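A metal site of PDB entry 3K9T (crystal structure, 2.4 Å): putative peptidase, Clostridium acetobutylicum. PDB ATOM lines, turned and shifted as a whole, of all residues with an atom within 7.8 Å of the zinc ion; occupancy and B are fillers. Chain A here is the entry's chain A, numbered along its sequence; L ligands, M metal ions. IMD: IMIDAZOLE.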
ATOM      1  N   TYR A 128      -9.022  11.620  -9.875  1.00  0.00           N
ATOM      2  CA  TYR A 128      -8.032  10.710  -9.266  1.00  0.00           C
ATOM      3  C   TYR A 128      -6.903  11.511  -8.622  1.00  0.00           C
ATOM      4  O   TYR A 128      -6.219  12.265  -9.276  1.00  0.00           O
ATOM      5  CB  TYR A 128      -7.470   9.752 -10.328  1.00  0.00           C
ATOM      6  CG  TYR A 128      -6.256   8.941  -9.931  1.00  0.00           C
ATOM      7  CD1 TYR A 128      -6.266   8.092  -8.820  1.00  0.00           C
ATOM      8  CD2 TYR A 128      -5.114   8.994 -10.693  1.00  0.00           C
ATOM      9  CE1 TYR A 128      -5.120   7.351  -8.469  1.00  0.00           C
ATOM     10  CE2 TYR A 128      -3.968   8.263 -10.365  1.00  0.00           C
ATOM     11  CZ  TYR A 128      -3.978   7.467  -9.249  1.00  0.00           C
ATOM     12  OH  TYR A 128      -2.835   6.743  -9.011  1.00  0.00           O
ATOM     13  N   TYR A 187       3.194   0.040 -16.030  1.00  0.00           N
ATOM     14  CA  TYR A 187       3.046   0.381 -14.614  1.00  0.00           C
ATOM     15  C   TYR A 187       1.709  -0.058 -13.979  1.00  0.00           C
ATOM     16  O   TYR A 187       0.633   0.066 -14.566  1.00  0.00           O
ATOM     17  CB  TYR A 187       3.410   1.870 -14.374  1.00  0.00           C
ATOM     18  CG  TYR A 187       2.651   2.854 -15.212  1.00  0.00           C
ATOM     19  CD1 TYR A 187       1.418   3.293 -14.813  1.00  0.00           C
ATOM     20  CD2 TYR A 187       3.160   3.352 -16.408  1.00  0.00           C
ATOM     21  CE1 TYR A 187       0.691   4.165 -15.547  1.00  0.00           C
ATOM     22  CE2 TYR A 187       2.444   4.266 -17.156  1.00  0.00           C
ATOM     23  CZ  TYR A 187       1.205   4.659 -16.727  1.00  0.00           C
ATOM     24  OH  TYR A 187       0.413   5.556 -17.438  1.00  0.00           O
ATOM     25  N   CYS A 189       0.380   0.764 -10.783  1.00  0.00           N
ATOM     26  CA  CYS A 189      -0.019   1.557  -9.635  1.00  0.00           C
ATOM     27  C   CYS A 189      -1.370   2.282  -9.758  1.00  0.00           C
ATOM     28  O   CYS A 189      -1.922   2.727  -8.748  1.00  0.00           O
ATOM     29  CB  CYS A 189       1.077   2.582  -9.366  1.00  0.00           C
ATOM     30  SG  CYS A 189       1.410   3.651 -10.799  1.00  0.00           S
ATOM     31  N   HIS A 190      -1.893   2.430 -10.971  1.00  0.00           N
ATOM     32  CA  HIS A 190      -3.196   3.090 -11.120  1.00  0.00           C
ATOM     33  C   HIS A 190      -4.363   2.159 -10.794  1.00  0.00           C
ATOM     34  O   HIS A 190      -4.384   1.006 -11.259  1.00  0.00           O
ATOM     35  CB  HIS A 190      -3.373   3.609 -12.522  1.00  0.00           C
ATOM     36  CG  HIS A 190      -2.551   4.810 -12.825  1.00  0.00           C
ATOM     37  ND1 HIS A 190      -1.239   4.946 -12.410  1.00  0.00           N
ATOM     38  CD2 HIS A 190      -2.835   5.928 -13.543  1.00  0.00           C
ATOM     39  CE1 HIS A 190      -0.769   6.088 -12.860  1.00  0.00           C
ATOM     40  NE2 HIS A 190      -1.714   6.701 -13.550  1.00  0.00           N
ATOM     41  N   MET A 193      -8.979   2.821 -13.464  1.00  0.00           N
ATOM     42  CA  MET A 193      -8.946   3.609 -14.698  1.00  0.00           C
ATOM     43  C   MET A 193      -8.384   2.666 -15.775  1.00  0.00           C
ATOM     44  O   MET A 193      -7.483   1.855 -15.502  1.00  0.00           O
ATOM     45  CB  MET A 193      -8.089   4.862 -14.543  1.00  0.00           C
ATOM     46  CG  MET A 193      -8.652   5.886 -13.529  1.00  0.00           C
ATOM     47  SD  MET A 193      -7.294   7.143 -13.091  1.00  0.00           S
ATOM     48  CE  MET A 193      -6.199   6.011 -11.908  1.00  0.00           C
ATOM     49  N   ASN A 195      -7.505   3.324 -19.714  1.00  0.00           N
ATOM     50  CA  ASN A 195      -6.424   3.674 -20.627  1.00  0.00           C
ATOM     51  C   ASN A 195      -5.119   3.879 -19.849  1.00  0.00           C
ATOM     52  O   ASN A 195      -4.044   3.325 -20.194  1.00  0.00           O
ATOM     53  CB  ASN A 195      -6.765   4.887 -21.500  1.00  0.00           C
ATOM     54  CG  ASN A 195      -6.183   4.768 -22.946  1.00  0.00           C
ATOM     55  OD1 ASN A 195      -6.004   3.667 -23.465  1.00  0.00           O
ATOM     56  ND2 ASN A 195      -5.904   5.902 -23.592  1.00  0.00           N
ATOM     57  N   ASP A 196      -5.218   4.622 -18.749  1.00  0.00           N
ATOM     58  CA  ASP A 196      -4.088   4.852 -17.853  1.00  0.00           C
ATOM     59  C   ASP A 196      -4.391   4.203 -16.477  1.00  0.00           C
ATOM     60  O   ASP A 196      -5.042   4.849 -15.663  1.00  0.00           O
ATOM     61  CB  ASP A 196      -3.874   6.372 -17.741  1.00  0.00           C
ATOM     62  CG  ASP A 196      -2.781   6.751 -16.776  1.00  0.00           C
ATOM     63  OD1 ASP A 196      -1.871   5.920 -16.594  1.00  0.00           O
ATOM     64  OD2 ASP A 196      -2.827   7.852 -16.173  1.00  0.00           O
ATOM     65  N   ASN A 197      -3.980   2.949 -16.195  1.00  0.00           N
ATOM     66  CA  ASN A 197      -3.168   2.107 -17.099  1.00  0.00           C
ATOM     67  C   ASN A 197      -3.422   0.600 -17.069  1.00  0.00           C
ATOM     68  O   ASN A 197      -2.459  -0.189 -17.029  1.00  0.00           O
ATOM     69  CB  ASN A 197      -1.651   2.320 -16.900  1.00  0.00           C
ATOM     70  CG  ASN A 197      -0.811   1.559 -17.925  1.00  0.00           C
ATOM     71  OD1 ASN A 197      -1.175   1.448 -19.100  1.00  0.00           O
ATOM     72  ND2 ASN A 197       0.327   1.006 -17.476  1.00  0.00           N
ATOM     73  N   GLU A 227       4.724   2.907 -11.263  1.00  0.00           N
ATOM     74  CA  GLU A 227       5.456   3.937 -11.976  1.00  0.00           C
ATOM     75  C   GLU A 227       6.492   4.651 -11.089  1.00  0.00           C
ATOM     76  O   GLU A 227       6.306   4.841  -9.898  1.00  0.00           O
ATOM     77  CB  GLU A 227       4.544   4.963 -12.633  1.00  0.00           C
ATOM     78  CG  GLU A 227       5.282   5.825 -13.697  1.00  0.00           C
ATOM     79  CD  GLU A 227       4.399   6.828 -14.404  1.00  0.00           C
ATOM     80  OE1 GLU A 227       3.767   7.626 -13.695  1.00  0.00           O
ATOM     81  OE2 GLU A 227       4.346   6.855 -15.655  1.00  0.00           O
ATOM     82  N   THR A 252       1.647   2.161 -22.327  1.00  0.00           N
ATOM     83  CA  THR A 252       0.587   2.755 -21.551  1.00  0.00           C
ATOM     84  C   THR A 252      -0.397   3.375 -22.534  1.00  0.00           C
ATOM     85  O   THR A 252      -0.044   3.596 -23.689  1.00  0.00           O
ATOM     86  CB  THR A 252       1.136   3.809 -20.598  1.00  0.00           C
ATOM     87  OG1 THR A 252       0.042   4.409 -19.921  1.00  0.00           O
ATOM     88  CG2 THR A 252       1.939   4.895 -21.315  1.00  0.00           C
ATOM     89  N   CYS A 253      -1.614   3.618 -22.061  1.00  0.00           N
ATOM     90  CA  CYS A 253      -2.632   4.316 -22.866  1.00  0.00           C
ATOM     91  C   CYS A 253      -2.813   3.732 -24.258  1.00  0.00           C
ATOM     92  O   CYS A 253      -2.860   4.479 -25.226  1.00  0.00           O
ATOM     93  CB  CYS A 253      -2.270   5.799 -22.981  1.00  0.00           C
ATOM     94  SG  CYS A 253      -2.244   6.654 -21.376  1.00  0.00           S
ATOM     95  N   GLY A 296       6.543  12.281 -18.215  1.00  0.00           N
ATOM     96  CA  GLY A 296       5.595  11.297 -18.715  1.00  0.00           C
ATOM     97  C   GLY A 296       5.714  10.018 -17.912  1.00  0.00           C
ATOM     98  O   GLY A 296       5.471  10.024 -16.721  1.00  0.00           O
ATOM     99  N   TYR A 319      -1.273  10.001 -22.431  1.00  0.00           N
ATOM    100  CA  TYR A 319      -1.649  10.614 -21.141  1.00  0.00           C
ATOM    101  C   TYR A 319      -1.728  12.151 -21.295  1.00  0.00           C
ATOM    102  O   TYR A 319      -0.882  12.769 -21.930  1.00  0.00           O
ATOM    103  CB  TYR A 319      -0.682  10.211 -19.989  1.00  0.00           C
ATOM    104  CG  TYR A 319       0.764  10.092 -20.408  1.00  0.00           C
ATOM    105  CD1 TYR A 319       1.542  11.209 -20.683  1.00  0.00           C
ATOM    106  CD2 TYR A 319       1.365   8.836 -20.541  1.00  0.00           C
ATOM    107  CE1 TYR A 319       2.867  11.085 -21.086  1.00  0.00           C
ATOM    108  CE2 TYR A 319       2.708   8.711 -20.931  1.00  0.00           C
ATOM    109  CZ  TYR A 319       3.449   9.821 -21.210  1.00  0.00           C
ATOM    110  OH  TYR A 319       4.769   9.677 -21.621  1.00  0.00           O
ATOM    111  N   GLY A 320      -2.781  12.741 -20.723  1.00  0.00           N
ATOM    112  CA  GLY A 320      -3.129  14.122 -20.994  1.00  0.00           C
ATOM    113  C   GLY A 320      -4.435  14.168 -21.749  1.00  0.00           C
ATOM    114  O   GLY A 320      -5.074  15.202 -21.830  1.00  0.00           O
ATOM    115  N   PHE A 321      -4.852  13.040 -22.326  1.00  0.00           N
ATOM    116  CA  PHE A 321      -6.139  12.927 -23.000  1.00  0.00           C
ATOM    117  C   PHE A 321      -7.327  13.375 -22.129  1.00  0.00           C
ATOM    118  O   PHE A 321      -7.297  13.342 -20.885  1.00  0.00           O
ATOM    119  CB  PHE A 321      -6.341  11.500 -23.520  1.00  0.00           C
ATOM    120  CG  PHE A 321      -6.467  10.447 -22.425  1.00  0.00           C
ATOM    121  CD1 PHE A 321      -7.706  10.163 -21.851  1.00  0.00           C
ATOM    122  CD2 PHE A 321      -5.374   9.701 -22.024  1.00  0.00           C
ATOM    123  CE1 PHE A 321      -7.829   9.216 -20.871  1.00  0.00           C
ATOM    124  CE2 PHE A 321      -5.494   8.730 -21.050  1.00  0.00           C
ATOM    125  CZ  PHE A 321      -6.726   8.483 -20.482  1.00  0.00           C
ATOM    126  N   TYR A 324      -8.484  11.833 -18.695  1.00  0.00           N
ATOM    127  CA  TYR A 324      -7.432  11.093 -18.018  1.00  0.00           C
ATOM    128  C   TYR A 324      -7.377  11.547 -16.547  1.00  0.00           C
ATOM    129  O   TYR A 324      -7.789  12.657 -16.209  1.00  0.00           O
ATOM    130  CB  TYR A 324      -6.095  11.218 -18.755  1.00  0.00           C
ATOM    131  CG  TYR A 324      -5.067  12.051 -18.106  1.00  0.00           C
ATOM    132  CD1 TYR A 324      -5.206  13.413 -18.032  1.00  0.00           C
ATOM    133  CD2 TYR A 324      -3.880  11.467 -17.603  1.00  0.00           C
ATOM    134  CE1 TYR A 324      -4.259  14.190 -17.419  1.00  0.00           C
ATOM    135  CE2 TYR A 324      -2.912  12.229 -17.005  1.00  0.00           C
ATOM    136  CZ  TYR A 324      -3.116  13.609 -16.914  1.00  0.00           C
ATOM    137  OH  TYR A 324      -2.189  14.443 -16.340  1.00  0.00           O
ATOM    138  N   HIS A 325      -6.958  10.639 -15.681  1.00  0.00           N
ATOM    139  CA  HIS A 325      -6.962  10.835 -14.236  1.00  0.00           C
ATOM    140  C   HIS A 325      -8.354  11.175 -13.687  1.00  0.00           C
ATOM    141  O   HIS A 325      -8.488  11.857 -12.705  1.00  0.00           O
ATOM    142  CB  HIS A 325      -5.868  11.827 -13.827  1.00  0.00           C
ATOM    143  CG  HIS A 325      -4.491  11.227 -13.865  1.00  0.00           C
ATOM    144  ND1 HIS A 325      -3.391  11.839 -13.316  1.00  0.00           N
ATOM    145  CD2 HIS A 325      -4.049  10.047 -14.360  1.00  0.00           C
ATOM    146  CE1 HIS A 325      -2.334  11.080 -13.493  1.00  0.00           C
ATOM    147  NE2 HIS A 325      -2.710   9.978 -14.126  1.00  0.00           N
ATOM    148  N   ASP A 329     -12.173   7.781 -17.664  1.00  0.00           N
ATOM    149  CA  ASP A 329     -11.315   6.731 -18.181  1.00  0.00           C
ATOM    150  C   ASP A 329     -11.787   5.361 -17.639  1.00  0.00           C
ATOM    151  O   ASP A 329     -11.103   4.701 -16.840  1.00  0.00           O
ATOM    152  CB  ASP A 329      -9.860   6.992 -17.759  1.00  0.00           C
ATOM    153  CG  ASP A 329      -8.870   6.029 -18.427  1.00  0.00           C
ATOM    154  OD1 ASP A 329      -9.309   5.244 -19.287  1.00  0.00           O
ATOM    155  OD2 ASP A 329      -7.667   6.046 -18.083  1.00  0.00           O
HETATM  156  N1  IMD L   1       2.297   8.419 -16.222  1.00  0.00           N
HETATM  157  C2  IMD L   1       1.314   7.764 -15.566  1.00  0.00           C
HETATM  158  N3  IMD L   1       0.206   8.486 -15.668  1.00  0.00           N
HETATM  159  C4  IMD L   1       0.463   9.590 -16.394  1.00  0.00           C
HETATM  160  C5  IMD L   1       1.799   9.550 -16.753  1.00  0.00           C
HETATM  161 ZN    ZN M   1      -1.614   8.355 -14.743  1.00  0.00          ZN
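The backbone carbonyl oxygen (O) of His 325 lies within hydrogen-bond range of the backbone NH (N) of Tyr 128 (2.9 Å). The side-chain hydroxyl (OH) of Tyr 187 sits at hydrogen-bond distance from the side-chain carboxylate (OD1) of Asp 196, at 2.5 Å. The side-chain sulfur (SG) of Cys 189 sits at hydrogen-bond distance from a ring nitrogen (ND1) of His 190, at 3.4 Å. N of Asp 196 is in hydrogen-bond range of OD2 of Asp 329, at 2.9 Å.
The zinc ion is bound by OD2 of Asp 196, 1.9 Å away. The zinc ion is bound by NE2 of His 190, 2.0 Å away. The zinc ion is bound by a nitrogen (N3) of the ligand (2.0 Å). A ring nitrogen (NE2) of His 325 is bound to the zinc ion (2.1 Å). The zinc ion has four donor atoms within binding distance.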
